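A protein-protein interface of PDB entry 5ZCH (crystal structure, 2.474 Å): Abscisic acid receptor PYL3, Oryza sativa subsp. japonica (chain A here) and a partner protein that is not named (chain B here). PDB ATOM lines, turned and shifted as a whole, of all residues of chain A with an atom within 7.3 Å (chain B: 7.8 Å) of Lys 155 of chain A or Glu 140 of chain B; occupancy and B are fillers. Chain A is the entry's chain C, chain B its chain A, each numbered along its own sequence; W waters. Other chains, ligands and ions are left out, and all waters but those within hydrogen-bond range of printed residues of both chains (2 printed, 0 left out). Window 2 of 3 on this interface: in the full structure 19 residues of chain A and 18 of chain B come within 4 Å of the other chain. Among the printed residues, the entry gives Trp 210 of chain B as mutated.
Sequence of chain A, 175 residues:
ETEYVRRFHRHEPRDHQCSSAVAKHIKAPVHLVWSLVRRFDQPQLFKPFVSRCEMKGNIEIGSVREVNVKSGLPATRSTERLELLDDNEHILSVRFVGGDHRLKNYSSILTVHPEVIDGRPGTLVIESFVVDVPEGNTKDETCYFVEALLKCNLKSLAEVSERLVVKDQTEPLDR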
ATOM      1  N   LYS A  24      29.687  -7.075   4.871  1.00  0.00           N
ATOM      2  CA  LYS A  24      29.174  -6.607   3.591  1.00  0.00           C
ATOM      3  C   LYS A  24      30.098  -7.083   2.481  1.00  0.00           C
ATOM      4  O   LYS A  24      31.320  -6.929   2.582  1.00  0.00           O
ATOM      5  CB  LYS A  24      29.056  -5.078   3.571  1.00  0.00           C
ATOM      6  CG  LYS A  24      28.664  -4.502   2.221  1.00  0.00           C
ATOM      7  CD  LYS A  24      27.240  -4.882   1.854  1.00  0.00           C
ATOM      8  CE  LYS A  24      26.646  -3.902   0.856  1.00  0.00           C
ATOM      9  NZ  LYS A  24      25.325  -4.360   0.344  1.00  0.00           N
ATOM     10  N   ILE A  26      31.469  -6.584  -1.236  1.00  0.00           N
ATOM     11  CA  ILE A  26      31.655  -5.502  -2.196  1.00  0.00           C
ATOM     12  C   ILE A  26      32.240  -6.090  -3.470  1.00  0.00           C
ATOM     13  O   ILE A  26      33.230  -6.829  -3.421  1.00  0.00           O
ATOM     14  CB  ILE A  26      32.566  -4.394  -1.636  1.00  0.00           C
ATOM     15  CG1 ILE A  26      32.047  -3.911  -0.279  1.00  0.00           C
ATOM     16  CG2 ILE A  26      32.664  -3.240  -2.623  1.00  0.00           C
ATOM     17  CD1 ILE A  26      32.709  -2.643   0.217  1.00  0.00           C
ATOM     18  N   PHE A  46      33.126   7.944   2.033  1.00  0.00           N
ATOM     19  CA  PHE A  46      32.134   6.880   1.969  1.00  0.00           C
ATOM     20  C   PHE A  46      31.102   6.928   3.084  1.00  0.00           C
ATOM     21  O   PHE A  46      30.084   6.239   2.972  1.00  0.00           O
ATOM     22  CB  PHE A  46      32.821   5.504   1.984  1.00  0.00           C
ATOM     23  CG  PHE A  46      33.336   5.092   3.336  1.00  0.00           C
ATOM     24  CD1 PHE A  46      34.551   5.565   3.803  1.00  0.00           C
ATOM     25  CD2 PHE A  46      32.609   4.224   4.137  1.00  0.00           C
ATOM     26  CE1 PHE A  46      35.029   5.185   5.044  1.00  0.00           C
ATOM     27  CE2 PHE A  46      33.082   3.841   5.379  1.00  0.00           C
ATOM     28  CZ  PHE A  46      34.294   4.322   5.832  1.00  0.00           C
ATOM     29  N   PRO A  48      27.992   8.394   4.817  1.00  0.00           N
ATOM     30  CA  PRO A  48      26.947   9.338   4.395  1.00  0.00           C
ATOM     31  C   PRO A  48      26.555  10.347   5.461  1.00  0.00           C
ATOM     32  O   PRO A  48      25.899  11.344   5.129  1.00  0.00           O
ATOM     33  CB  PRO A  48      25.757   8.424   4.049  1.00  0.00           C
ATOM     34  CG  PRO A  48      26.212   7.008   4.312  1.00  0.00           C
ATOM     35  CD  PRO A  48      27.442   7.072   5.149  1.00  0.00           C
ATOM     36  N   PHE A  49      26.928  10.126   6.723  1.00  0.00           N
ATOM     37  CA  PHE A  49      26.512  11.008   7.803  1.00  0.00           C
ATOM     38  C   PHE A  49      27.478  12.155   8.057  1.00  0.00           C
ATOM     39  O   PHE A  49      27.100  13.124   8.723  1.00  0.00           O
ATOM     40  CB  PHE A  49      26.346  10.215   9.103  1.00  0.00           C
ATOM     41  CG  PHE A  49      25.448   9.023   8.976  1.00  0.00           C
ATOM     42  CD1 PHE A  49      24.087   9.185   8.787  1.00  0.00           C
ATOM     43  CD2 PHE A  49      25.963   7.740   9.049  1.00  0.00           C
ATOM     44  CE1 PHE A  49      23.257   8.090   8.670  1.00  0.00           C
ATOM     45  CE2 PHE A  49      25.136   6.639   8.933  1.00  0.00           C
ATOM     46  CZ  PHE A  49      23.781   6.816   8.742  1.00  0.00           C
ATOM     47  N   LEU A 149      23.612   2.075  11.820  1.00  0.00           N
ATOM     48  CA  LEU A 149      24.530   3.064  11.268  1.00  0.00           C
ATOM     49  C   LEU A 149      25.662   2.401  10.492  1.00  0.00           C
ATOM     50  O   LEU A 149      26.065   2.889   9.430  1.00  0.00           O
ATOM     51  CB  LEU A 149      25.091   3.942  12.386  1.00  0.00           C
ATOM     52  CG  LEU A 149      24.080   4.793  13.157  1.00  0.00           C
ATOM     53  CD1 LEU A 149      24.754   5.499  14.321  1.00  0.00           C
ATOM     54  CD2 LEU A 149      23.408   5.797  12.235  1.00  0.00           C
ATOM     55  N   LEU A 150      26.186   1.284  11.005  1.00  0.00           N
ATOM     56  CA  LEU A 150      27.307   0.623  10.345  1.00  0.00           C
ATOM     57  C   LEU A 150      26.888   0.011   9.014  1.00  0.00           C
ATOM     58  O   LEU A 150      27.644   0.063   8.037  1.00  0.00           O
ATOM     59  CB  LEU A 150      27.902  -0.443  11.265  1.00  0.00           C
ATOM     60  CG  LEU A 150      28.580   0.075  12.533  1.00  0.00           C
ATOM     61  CD1 LEU A 150      29.277  -1.055  13.274  1.00  0.00           C
ATOM     62  CD2 LEU A 150      29.561   1.185  12.196  1.00  0.00           C
ATOM     63  N   LYS A 151      25.691  -0.578   8.958  1.00  0.00           N
ATOM     64  CA  LYS A 151      25.201  -1.121   7.694  1.00  0.00           C
ATOM     65  C   LYS A 151      24.989  -0.015   6.669  1.00  0.00           C
ATOM     66  O   LYS A 151      25.246  -0.206   5.475  1.00  0.00           O
ATOM     67  CB  LYS A 151      23.911  -1.907   7.922  1.00  0.00           C
ATOM     68  CG  LYS A 151      24.110  -3.208   8.684  1.00  0.00           C
ATOM     69  CD  LYS A 151      22.826  -4.018   8.754  1.00  0.00           C
ATOM     70  CE  LYS A 151      22.766  -4.836  10.035  1.00  0.00           C
ATOM     71  NZ  LYS A 151      23.090  -6.269   9.797  1.00  0.00           N
ATOM     72  N   CYS A 152      24.522   1.152   7.118  1.00  0.00           N
ATOM     73  CA  CYS A 152      24.410   2.296   6.220  1.00  0.00           C
ATOM     74  C   CYS A 152      25.783   2.758   5.747  1.00  0.00           C
ATOM     75  O   CYS A 152      25.945   3.153   4.586  1.00  0.00           O
ATOM     76  CB  CYS A 152      23.668   3.436   6.916  1.00  0.00           C
ATOM     77  SG  CYS A 152      23.080   4.738   5.812  1.00  0.00           S
ATOM     78  N   ASN A 153      26.781   2.717   6.632  1.00  0.00           N
ATOM     79  CA  ASN A 153      28.140   3.078   6.243  1.00  0.00           C
ATOM     80  C   ASN A 153      28.691   2.103   5.209  1.00  0.00           C
ATOM     81  O   ASN A 153      29.241   2.514   4.180  1.00  0.00           O
ATOM     82  CB  ASN A 153      29.045   3.120   7.475  1.00  0.00           C
ATOM     83  CG  ASN A 153      28.969   4.442   8.212  1.00  0.00           C
ATOM     84  OD1 ASN A 153      28.371   5.402   7.732  1.00  0.00           O
ATOM     85  ND2 ASN A 153      29.579   4.495   9.390  1.00  0.00           N
ATOM     86  N   LEU A 154      28.553   0.801   5.470  1.00  0.00           N
ATOM     87  CA  LEU A 154      29.122  -0.202   4.574  1.00  0.00           C
ATOM     88  C   LEU A 154      28.396  -0.234   3.235  1.00  0.00           C
ATOM     89  O   LEU A 154      29.021  -0.465   2.193  1.00  0.00           O
ATOM     90  CB  LEU A 154      29.086  -1.579   5.239  1.00  0.00           C
ATOM     91  CG  LEU A 154      30.007  -1.752   6.449  1.00  0.00           C
ATOM     92  CD1 LEU A 154      30.054  -3.206   6.893  1.00  0.00           C
ATOM     93  CD2 LEU A 154      31.405  -1.237   6.135  1.00  0.00           C
ATOM     94  N   LYS A 155      27.080  -0.012   3.238  1.00  0.00           N
ATOM     95  CA  LYS A 155      26.344   0.028   1.979  1.00  0.00           C
ATOM     96  C   LYS A 155      26.797   1.200   1.120  1.00  0.00           C
ATOM     97  O   LYS A 155      26.908   1.078  -0.107  1.00  0.00           O
ATOM     98  CB  LYS A 155      24.841   0.106   2.240  1.00  0.00           C
ATOM     99  CG  LYS A 155      24.001   0.054   0.975  1.00  0.00           C
ATOM    100  CD  LYS A 155      22.595   0.573   1.212  1.00  0.00           C
ATOM    101  CE  LYS A 155      21.718  -0.479   1.871  1.00  0.00           C
ATOM    102  NZ  LYS A 155      20.270  -0.215   1.639  1.00  0.00           N
ATOM    103  N   SER A 156      27.067   2.347   1.747  1.00  0.00           N
ATOM    104  CA  SER A 156      27.579   3.489   0.999  1.00  0.00           C
ATOM    105  C   SER A 156      29.001   3.233   0.518  1.00  0.00           C
ATOM    106  O   SER A 156      29.373   3.649  -0.586  1.00  0.00           O
ATOM    107  CB  SER A 156      27.517   4.748   1.862  1.00  0.00           C
ATOM    108  OG  SER A 156      28.250   5.809   1.275  1.00  0.00           O
ATOM    109  N   LEU A 157      29.810   2.548   1.331  1.00  0.00           N
ATOM    110  CA  LEU A 157      31.151   2.175   0.897  1.00  0.00           C
ATOM    111  C   LEU A 157      31.098   1.232  -0.299  1.00  0.00           C
ATOM    112  O   LEU A 157      31.914   1.341  -1.222  1.00  0.00           O
ATOM    113  CB  LEU A 157      31.916   1.529   2.053  1.00  0.00           C
ATOM    114  CG  LEU A 157      33.225   0.820   1.696  1.00  0.00           C
ATOM    115  CD1 LEU A 157      34.256   1.810   1.170  1.00  0.00           C
ATOM    116  CD2 LEU A 157      33.767   0.056   2.895  1.00  0.00           C
ATOM    117  N   ALA A 158      30.142   0.302  -0.299  1.00  0.00           N
ATOM    118  CA  ALA A 158      30.006  -0.617  -1.424  1.00  0.00           C
ATOM    119  C   ALA A 158      29.625   0.122  -2.700  1.00  0.00           C
ATOM    120  O   ALA A 158      30.193  -0.134  -3.768  1.00  0.00           O
ATOM    121  CB  ALA A 158      28.974  -1.697  -1.101  1.00  0.00           C
ATOM    122  N   GLU A 159      28.670   1.051  -2.608  1.00  0.00           N
ATOM    123  CA  GLU A 159      28.229   1.773  -3.797  1.00  0.00           C
ATOM    124  C   GLU A 159      29.308   2.714  -4.319  1.00  0.00           C
ATOM    125  O   GLU A 159      29.399   2.934  -5.533  1.00  0.00           O
ATOM    126  CB  GLU A 159      26.941   2.538  -3.498  1.00  0.00           C
ATOM    127  CG  GLU A 159      25.699   1.659  -3.523  1.00  0.00           C
ATOM    128  CD  GLU A 159      24.447   2.395  -3.095  1.00  0.00           C
ATOM    129  OE1 GLU A 159      24.566   3.405  -2.370  1.00  0.00           O
ATOM    130  OE2 GLU A 159      23.341   1.961  -3.481  1.00  0.00           O
ATOM    131  N   VAL A 160      30.128   3.277  -3.432  1.00  0.00           N
ATOM    132  CA  VAL A 160      31.222   4.132  -3.884  1.00  0.00           C
ATOM    133  C   VAL A 160      32.348   3.289  -4.471  1.00  0.00           C
ATOM    134  O   VAL A 160      32.937   3.649  -5.497  1.00  0.00           O
ATOM    135  CB  VAL A 160      31.715   5.024  -2.730  1.00  0.00           C
ATOM    136  CG1 VAL A 160      32.982   5.765  -3.131  1.00  0.00           C
ATOM    137  CG2 VAL A 160      30.632   6.010  -2.321  1.00  0.00           C
ATOM    138  N   SER A 161      32.660   2.155  -3.838  1.00  0.00           N
ATOM    139  CA  SER A 161      33.703   1.278  -4.362  1.00  0.00           C
ATOM    140  C   SER A 161      33.317   0.719  -5.725  1.00  0.00           C
ATOM    141  O   SER A 161      34.174   0.552  -6.601  1.00  0.00           O
ATOM    142  CB  SER A 161      33.983   0.143  -3.378  1.00  0.00           C
ATOM    143  OG  SER A 161      34.564   0.632  -2.183  1.00  0.00           O
ATOM    144  N   GLU A 162      32.032   0.426  -5.925  1.00  0.00           N
ATOM    145  CA  GLU A 162      31.577  -0.192  -7.163  1.00  0.00           C
ATOM    146  C   GLU A 162      31.320   0.822  -8.268  1.00  0.00           C
ATOM    147  O   GLU A 162      31.106   0.420  -9.417  1.00  0.00           O
ATOM    148  CB  GLU A 162      30.307  -1.010  -6.912  1.00  0.00           C
ATOM    149  CG  GLU A 162      30.544  -2.306  -6.154  1.00  0.00           C
ATOM    150  CD  GLU A 162      29.261  -2.913  -5.624  1.00  0.00           C
ATOM    151  OE1 GLU A 162      28.174  -2.527  -6.107  1.00  0.00           O
ATOM    152  OE2 GLU A 162      29.337  -3.775  -4.724  1.00  0.00           O
ATOM    153  N   HIS B  63      15.943  16.964   6.624  1.00  0.00           N
ATOM    154  CA  HIS B  63      16.965  16.488   7.545  1.00  0.00           C
ATOM    155  C   HIS B  63      17.998  15.693   6.760  1.00  0.00           C
ATOM    156  O   HIS B  63      17.681  15.071   5.742  1.00  0.00           O
ATOM    157  CB  HIS B  63      16.367  15.633   8.668  1.00  0.00           C
ATOM    158  CG  HIS B  63      15.491  14.521   8.182  1.00  0.00           C
ATOM    159  ND1 HIS B  63      14.116  14.568   8.261  1.00  0.00           N
ATOM    160  CD2 HIS B  63      15.795  13.331   7.612  1.00  0.00           C
ATOM    161  CE1 HIS B  63      13.610  13.455   7.761  1.00  0.00           C
ATOM    162  NE2 HIS B  63      14.607  12.688   7.360  1.00  0.00           N
ATOM    163  N   SER B 119      13.993   8.714  -4.543  1.00  0.00           N
ATOM    164  CA  SER B 119      14.822   7.525  -4.399  1.00  0.00           C
ATOM    165  C   SER B 119      15.402   7.033  -5.718  1.00  0.00           C
ATOM    166  O   SER B 119      16.145   6.047  -5.717  1.00  0.00           O
ATOM    167  CB  SER B 119      14.012   6.399  -3.750  1.00  0.00           C
ATOM    168  OG  SER B 119      13.533   6.786  -2.474  1.00  0.00           O
ATOM    169  N   PRO B 136      18.960   8.498  -8.001  1.00  0.00           N
ATOM    170  CA  PRO B 136      18.357   9.156  -6.833  1.00  0.00           C
ATOM    171  C   PRO B 136      18.744  10.623  -6.730  1.00  0.00           C
ATOM    172  O   PRO B 136      19.820  11.041  -7.166  1.00  0.00           O
ATOM    173  CB  PRO B 136      18.908   8.352  -5.650  1.00  0.00           C
ATOM    174  CG  PRO B 136      19.199   7.011  -6.216  1.00  0.00           C
ATOM    175  CD  PRO B 136      19.640   7.242  -7.633  1.00  0.00           C
ATOM    176  N   THR B 138      19.338  12.270  -3.965  1.00  0.00           N
ATOM    177  CA  THR B 138      20.373  12.455  -2.956  1.00  0.00           C
ATOM    178  C   THR B 138      20.641  11.118  -2.270  1.00  0.00           C
ATOM    179  O   THR B 138      20.130  10.072  -2.683  1.00  0.00           O
ATOM    180  CB  THR B 138      19.965  13.546  -1.958  1.00  0.00           C
ATOM    181  OG1 THR B 138      20.994  13.706  -0.973  1.00  0.00           O
ATOM    182  CG2 THR B 138      18.663  13.174  -1.278  1.00  0.00           C
ATOM    183  N   ALA B 139      21.446  11.164  -1.211  1.00  0.00           N
ATOM    184  CA  ALA B 139      21.896   9.977  -0.500  1.00  0.00           C
ATOM    185  C   ALA B 139      20.748   9.309   0.258  1.00  0.00           C
ATOM    186  O   ALA B 139      19.636   9.831   0.368  1.00  0.00           O
ATOM    187  CB  ALA B 139      23.028  10.332   0.464  1.00  0.00           C
ATOM    188  N   GLU B 140      21.048   8.117   0.786  1.00  0.00           N
ATOM    189  CA  GLU B 140      20.056   7.283   1.456  1.00  0.00           C
ATOM    190  C   GLU B 140      19.587   7.858   2.786  1.00  0.00           C
ATOM    191  O   GLU B 140      18.552   7.422   3.300  1.00  0.00           O
ATOM    192  CB  GLU B 140      20.645   5.894   1.707  1.00  0.00           C
ATOM    193  CG  GLU B 140      20.100   4.779   0.841  1.00  0.00           C
ATOM    194  CD  GLU B 140      20.419   3.412   1.415  1.00  0.00           C
ATOM    195  OE1 GLU B 140      21.339   3.325   2.257  1.00  0.00           O
ATOM    196  OE2 GLU B 140      19.752   2.429   1.029  1.00  0.00           O
ATOM    197  N   ASN B 141      20.312   8.821   3.354  1.00  0.00           N
ATOM    198  CA  ASN B 141      20.035   9.313   4.698  1.00  0.00           C
ATOM    199  C   ASN B 141      19.398  10.698   4.718  1.00  0.00           C
ATOM    200  O   ASN B 141      19.345  11.324   5.782  1.00  0.00           O
ATOM    201  CB  ASN B 141      21.322   9.327   5.524  1.00  0.00           C
ATOM    202  CG  ASN B 141      22.360  10.276   4.962  1.00  0.00           C
ATOM    203  OD1 ASN B 141      22.783  10.143   3.814  1.00  0.00           O
ATOM    204  ND2 ASN B 141      22.774  11.246   5.769  1.00  0.00           N
ATOM    205  N   VAL B 142      18.914  11.193   3.583  1.00  0.00           N
ATOM    206  CA  VAL B 142      18.297  12.511   3.504  1.00  0.00           C
ATOM    207  C   VAL B 142      16.791  12.344   3.363  1.00  0.00           C
ATOM    208  O   VAL B 142      16.317  11.478   2.618  1.00  0.00           O
ATOM    209  CB  VAL B 142      18.871  13.333   2.333  1.00  0.00           C
ATOM    210  CG1 VAL B 142      18.429  14.784   2.434  1.00  0.00           C
ATOM    211  CG2 VAL B 142      20.388  13.232   2.311  1.00  0.00           C
ATOM    212  N   GLY B 143      16.043  13.174   4.083  1.00  0.00           N
ATOM    213  CA  GLY B 143      14.595  13.144   4.029  1.00  0.00           C
ATOM    214  C   GLY B 143      13.985  14.501   4.307  1.00  0.00           C
ATOM    215  O   GLY B 143      14.704  15.503   4.378  1.00  0.00           O
ATOM    216  N   TRP B 210      17.403   6.457  15.640  1.00  0.00           N
ATOM    217  CA  TRP B 210      17.955   7.431  14.701  1.00  0.00           C
ATOM    218  C   TRP B 210      16.984   8.575  14.462  1.00  0.00           C
ATOM    219  O   TRP B 210      17.238   9.701  14.902  1.00  0.00           O
ATOM    220  CB  TRP B 210      18.327   6.697  13.403  1.00  0.00           C
ATOM    221  CG  TRP B 210      18.663   7.528  12.172  1.00  0.00           C
ATOM    222  CD1 TRP B 210      18.519   8.879  11.998  1.00  0.00           C
ATOM    223  CD2 TRP B 210      19.192   7.026  10.939  1.00  0.00           C
ATOM    224  NE1 TRP B 210      18.925   9.242  10.738  1.00  0.00           N
ATOM    225  CE2 TRP B 210      19.344   8.124  10.069  1.00  0.00           C
ATOM    226  CE3 TRP B 210      19.555   5.754  10.488  1.00  0.00           C
ATOM    227  CZ2 TRP B 210      19.843   7.987   8.775  1.00  0.00           C
ATOM    228  CZ3 TRP B 210      20.050   5.620   9.204  1.00  0.00           C
ATOM    229  CH2 TRP B 210      20.188   6.729   8.362  1.00  0.00           C
ATOM    230  N   GLY B 218      11.463  10.363   1.461  1.00  0.00           N
ATOM    231  CA  GLY B 218      12.863  10.005   1.356  1.00  0.00           C
ATOM    232  C   GLY B 218      13.272   9.016   2.428  1.00  0.00           C
ATOM    233  O   GLY B 218      12.477   8.145   2.798  1.00  0.00           O
ATOM    234  N   ASP B 219      14.498   9.144   2.941  1.00  0.00           N
ATOM    235  CA  ASP B 219      15.008   8.279   4.006  1.00  0.00           C
ATOM    236  C   ASP B 219      14.847   6.806   3.638  1.00  0.00           C
ATOM    237  O   ASP B 219      14.327   5.998   4.412  1.00  0.00           O
ATOM    238  CB  ASP B 219      14.320   8.582   5.339  1.00  0.00           C
ATOM    239  CG  ASP B 219      14.805   9.870   5.969  1.00  0.00           C
ATOM    240  OD1 ASP B 219      16.009   9.964   6.290  1.00  0.00           O
ATOM    241  OD2 ASP B 219      13.979  10.788   6.150  1.00  0.00           O
ATOM    242  N   ARG B 220      15.297   6.455   2.431  1.00  0.00           N
ATOM    243  CA  ARG B 220      15.043   5.114   1.918  1.00  0.00           C
ATOM    244  C   ARG B 220      15.811   4.034   2.672  1.00  0.00           C
ATOM    245  O   ARG B 220      15.457   2.855   2.559  1.00  0.00           O
ATOM    246  CB  ARG B 220      15.365   5.046   0.423  1.00  0.00           C
ATOM    247  CG  ARG B 220      16.754   5.515   0.045  1.00  0.00           C
ATOM    248  CD  ARG B 220      17.000   5.319  -1.445  1.00  0.00           C
ATOM    249  NE  ARG B 220      18.338   5.740  -1.851  1.00  0.00           N
ATOM    250  CZ  ARG B 220      18.669   6.991  -2.156  1.00  0.00           C
ATOM    251  NH1 ARG B 220      17.757   7.952  -2.100  1.00  0.00           N
ATOM    252  NH2 ARG B 220      19.912   7.282  -2.515  1.00  0.00           N
ATOM    253  N   TYR B 221      16.849   4.394   3.431  1.00  0.00           N
ATOM    254  CA  TYR B 221      17.516   3.382   4.246  1.00  0.00           C
ATOM    255  C   TYR B 221      16.624   2.916   5.391  1.00  0.00           C
ATOM    256  O   TYR B 221      16.601   1.725   5.719  1.00  0.00           O
ATOM    257  CB  TYR B 221      18.843   3.902   4.797  1.00  0.00           C
ATOM    258  CG  TYR B 221      19.512   2.883   5.695  1.00  0.00           C
ATOM    259  CD1 TYR B 221      20.215   1.812   5.157  1.00  0.00           C
ATOM    260  CD2 TYR B 221      19.409   2.969   7.078  1.00  0.00           C
ATOM    261  CE1 TYR B 221      20.815   0.869   5.970  1.00  0.00           C
ATOM    262  CE2 TYR B 221      20.004   2.029   7.900  1.00  0.00           C
ATOM    263  CZ  TYR B 221      20.706   0.981   7.339  1.00  0.00           C
ATOM    264  OH  TYR B 221      21.300   0.044   8.152  1.00  0.00           O
ATOM    265  N   LEU B 222      15.886   3.836   6.007  1.00  0.00           N
ATOM    266  CA  LEU B 222      15.059   3.519   7.166  1.00  0.00           C
ATOM    267  C   LEU B 222      13.715   2.902   6.792  1.00  0.00           C
ATOM    268  O   LEU B 222      12.864   2.732   7.671  1.00  0.00           O
ATOM    269  CB  LEU B 222      14.838   4.776   8.011  1.00  0.00           C
ATOM    270  CG  LEU B 222      16.026   5.198   8.877  1.00  0.00           C
ATOM    271  CD1 LEU B 222      15.693   6.446   9.680  1.00  0.00           C
ATOM    272  CD2 LEU B 222      16.452   4.060   9.795  1.00  0.00           C
ATOM    273  N   LYS B 223      13.507   2.567   5.524  1.00  0.00           N
ATOM    274  CA  LYS B 223      12.308   1.855   5.116  1.00  0.00           C
ATOM    275  C   LYS B 223      12.431   0.375   5.481  1.00  0.00           C
ATOM    276  O   LYS B 223      13.540  -0.162   5.552  1.00  0.00           O
ATOM    277  CB  LYS B 223      12.085   2.012   3.615  1.00  0.00           C
ATOM    278  CG  LYS B 223      11.776   3.440   3.188  1.00  0.00           C
ATOM    279  CD  LYS B 223      11.078   3.483   1.839  1.00  0.00           C
ATOM    280  CE  LYS B 223      10.924   4.913   1.343  1.00  0.00           C
ATOM    281  NZ  LYS B 223      10.354   5.806   2.391  1.00  0.00           N
HETATM  282  O   HOH W   1      23.957   4.587   2.533  1.00  0.00           O
HETATM  283  O   HOH W   2      24.191  12.598   2.516  1.00  0.00           O
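Water W1 lies within hydrogen-bond range of the side-chain carboxylate (OE1) of Glu 140 of chain B (2.9 Å) and the backbone carbonyl oxygen (O) of Cys 152 of chain A (3.2 Å). Water W2 bridges OD1 of Asn 141 of chain B and O of Pro 48 of chain A.
Printed residues of chain B within 4 Å of Lys 155 of chain A: Glu 140. Glu 140 of chain B touches just one residue of chain A: Lys 155 (2.8 Å). Printed residues of chain B within 4 Å of Cys 152 of chain A: Tyr 221 (3.6 Å). Of the printed residues of chain B, Phe 49 of chain A touches Asn 141 (3.9 Å) and Trp 210 (3.4 Å). Printed residues of chain A within 4 Å of Trp 210 of chain B: Phe 49 (3.4 Å). Printed residues of chain A within 4 Å of Asn 141 of chain B: Pro 48 (3.2 Å) and Phe 49 (3.9 Å). Of the printed residues of chain A, Tyr 221 of chain B touches Lys 151 (3.3 Å) and Cys 152 (3.6 Å). Gly 218 of chain B touches none of the printed residues of chain A. Ser 156 of chain A touches none of the printed residues of chain B.
The backbone carbonyl oxygen (O) of Glu 140 of chain B lies within hydrogen-bond range of the backbone NH (N) of Tyr 221 of chain B, at 3.5 Å.
Of the 16 printed residues of chain B, 4 touch a printed residue of chain A. Among the printed residues, Asp or Glu carboxylates within 4 Å of a Lys or Arg side-chain nitrogen of the other chain: Lys 155 of chain A with Glu 140 of chain B.
O of Pro 48 of chain A sits at hydrogen-bond distance from ND2 of Asn 141 of chain B (3.2 Å). The side-chain carboxylate (OE2) of Glu 140 of chain B is in salt-bridge range of the side-chain amino group (NZ) of Lys 155 of chain A (2.8 Å).
Among the printed residues, merely in contact across the chains: Lys 151 of chain A with Tyr 221 of chain B, Phe 49 of chain A with Trp 210 of chain B, Cys 152 of chain A with Tyr 221 of chain B and Phe 49 of chain A with Asn 141 of chain B.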
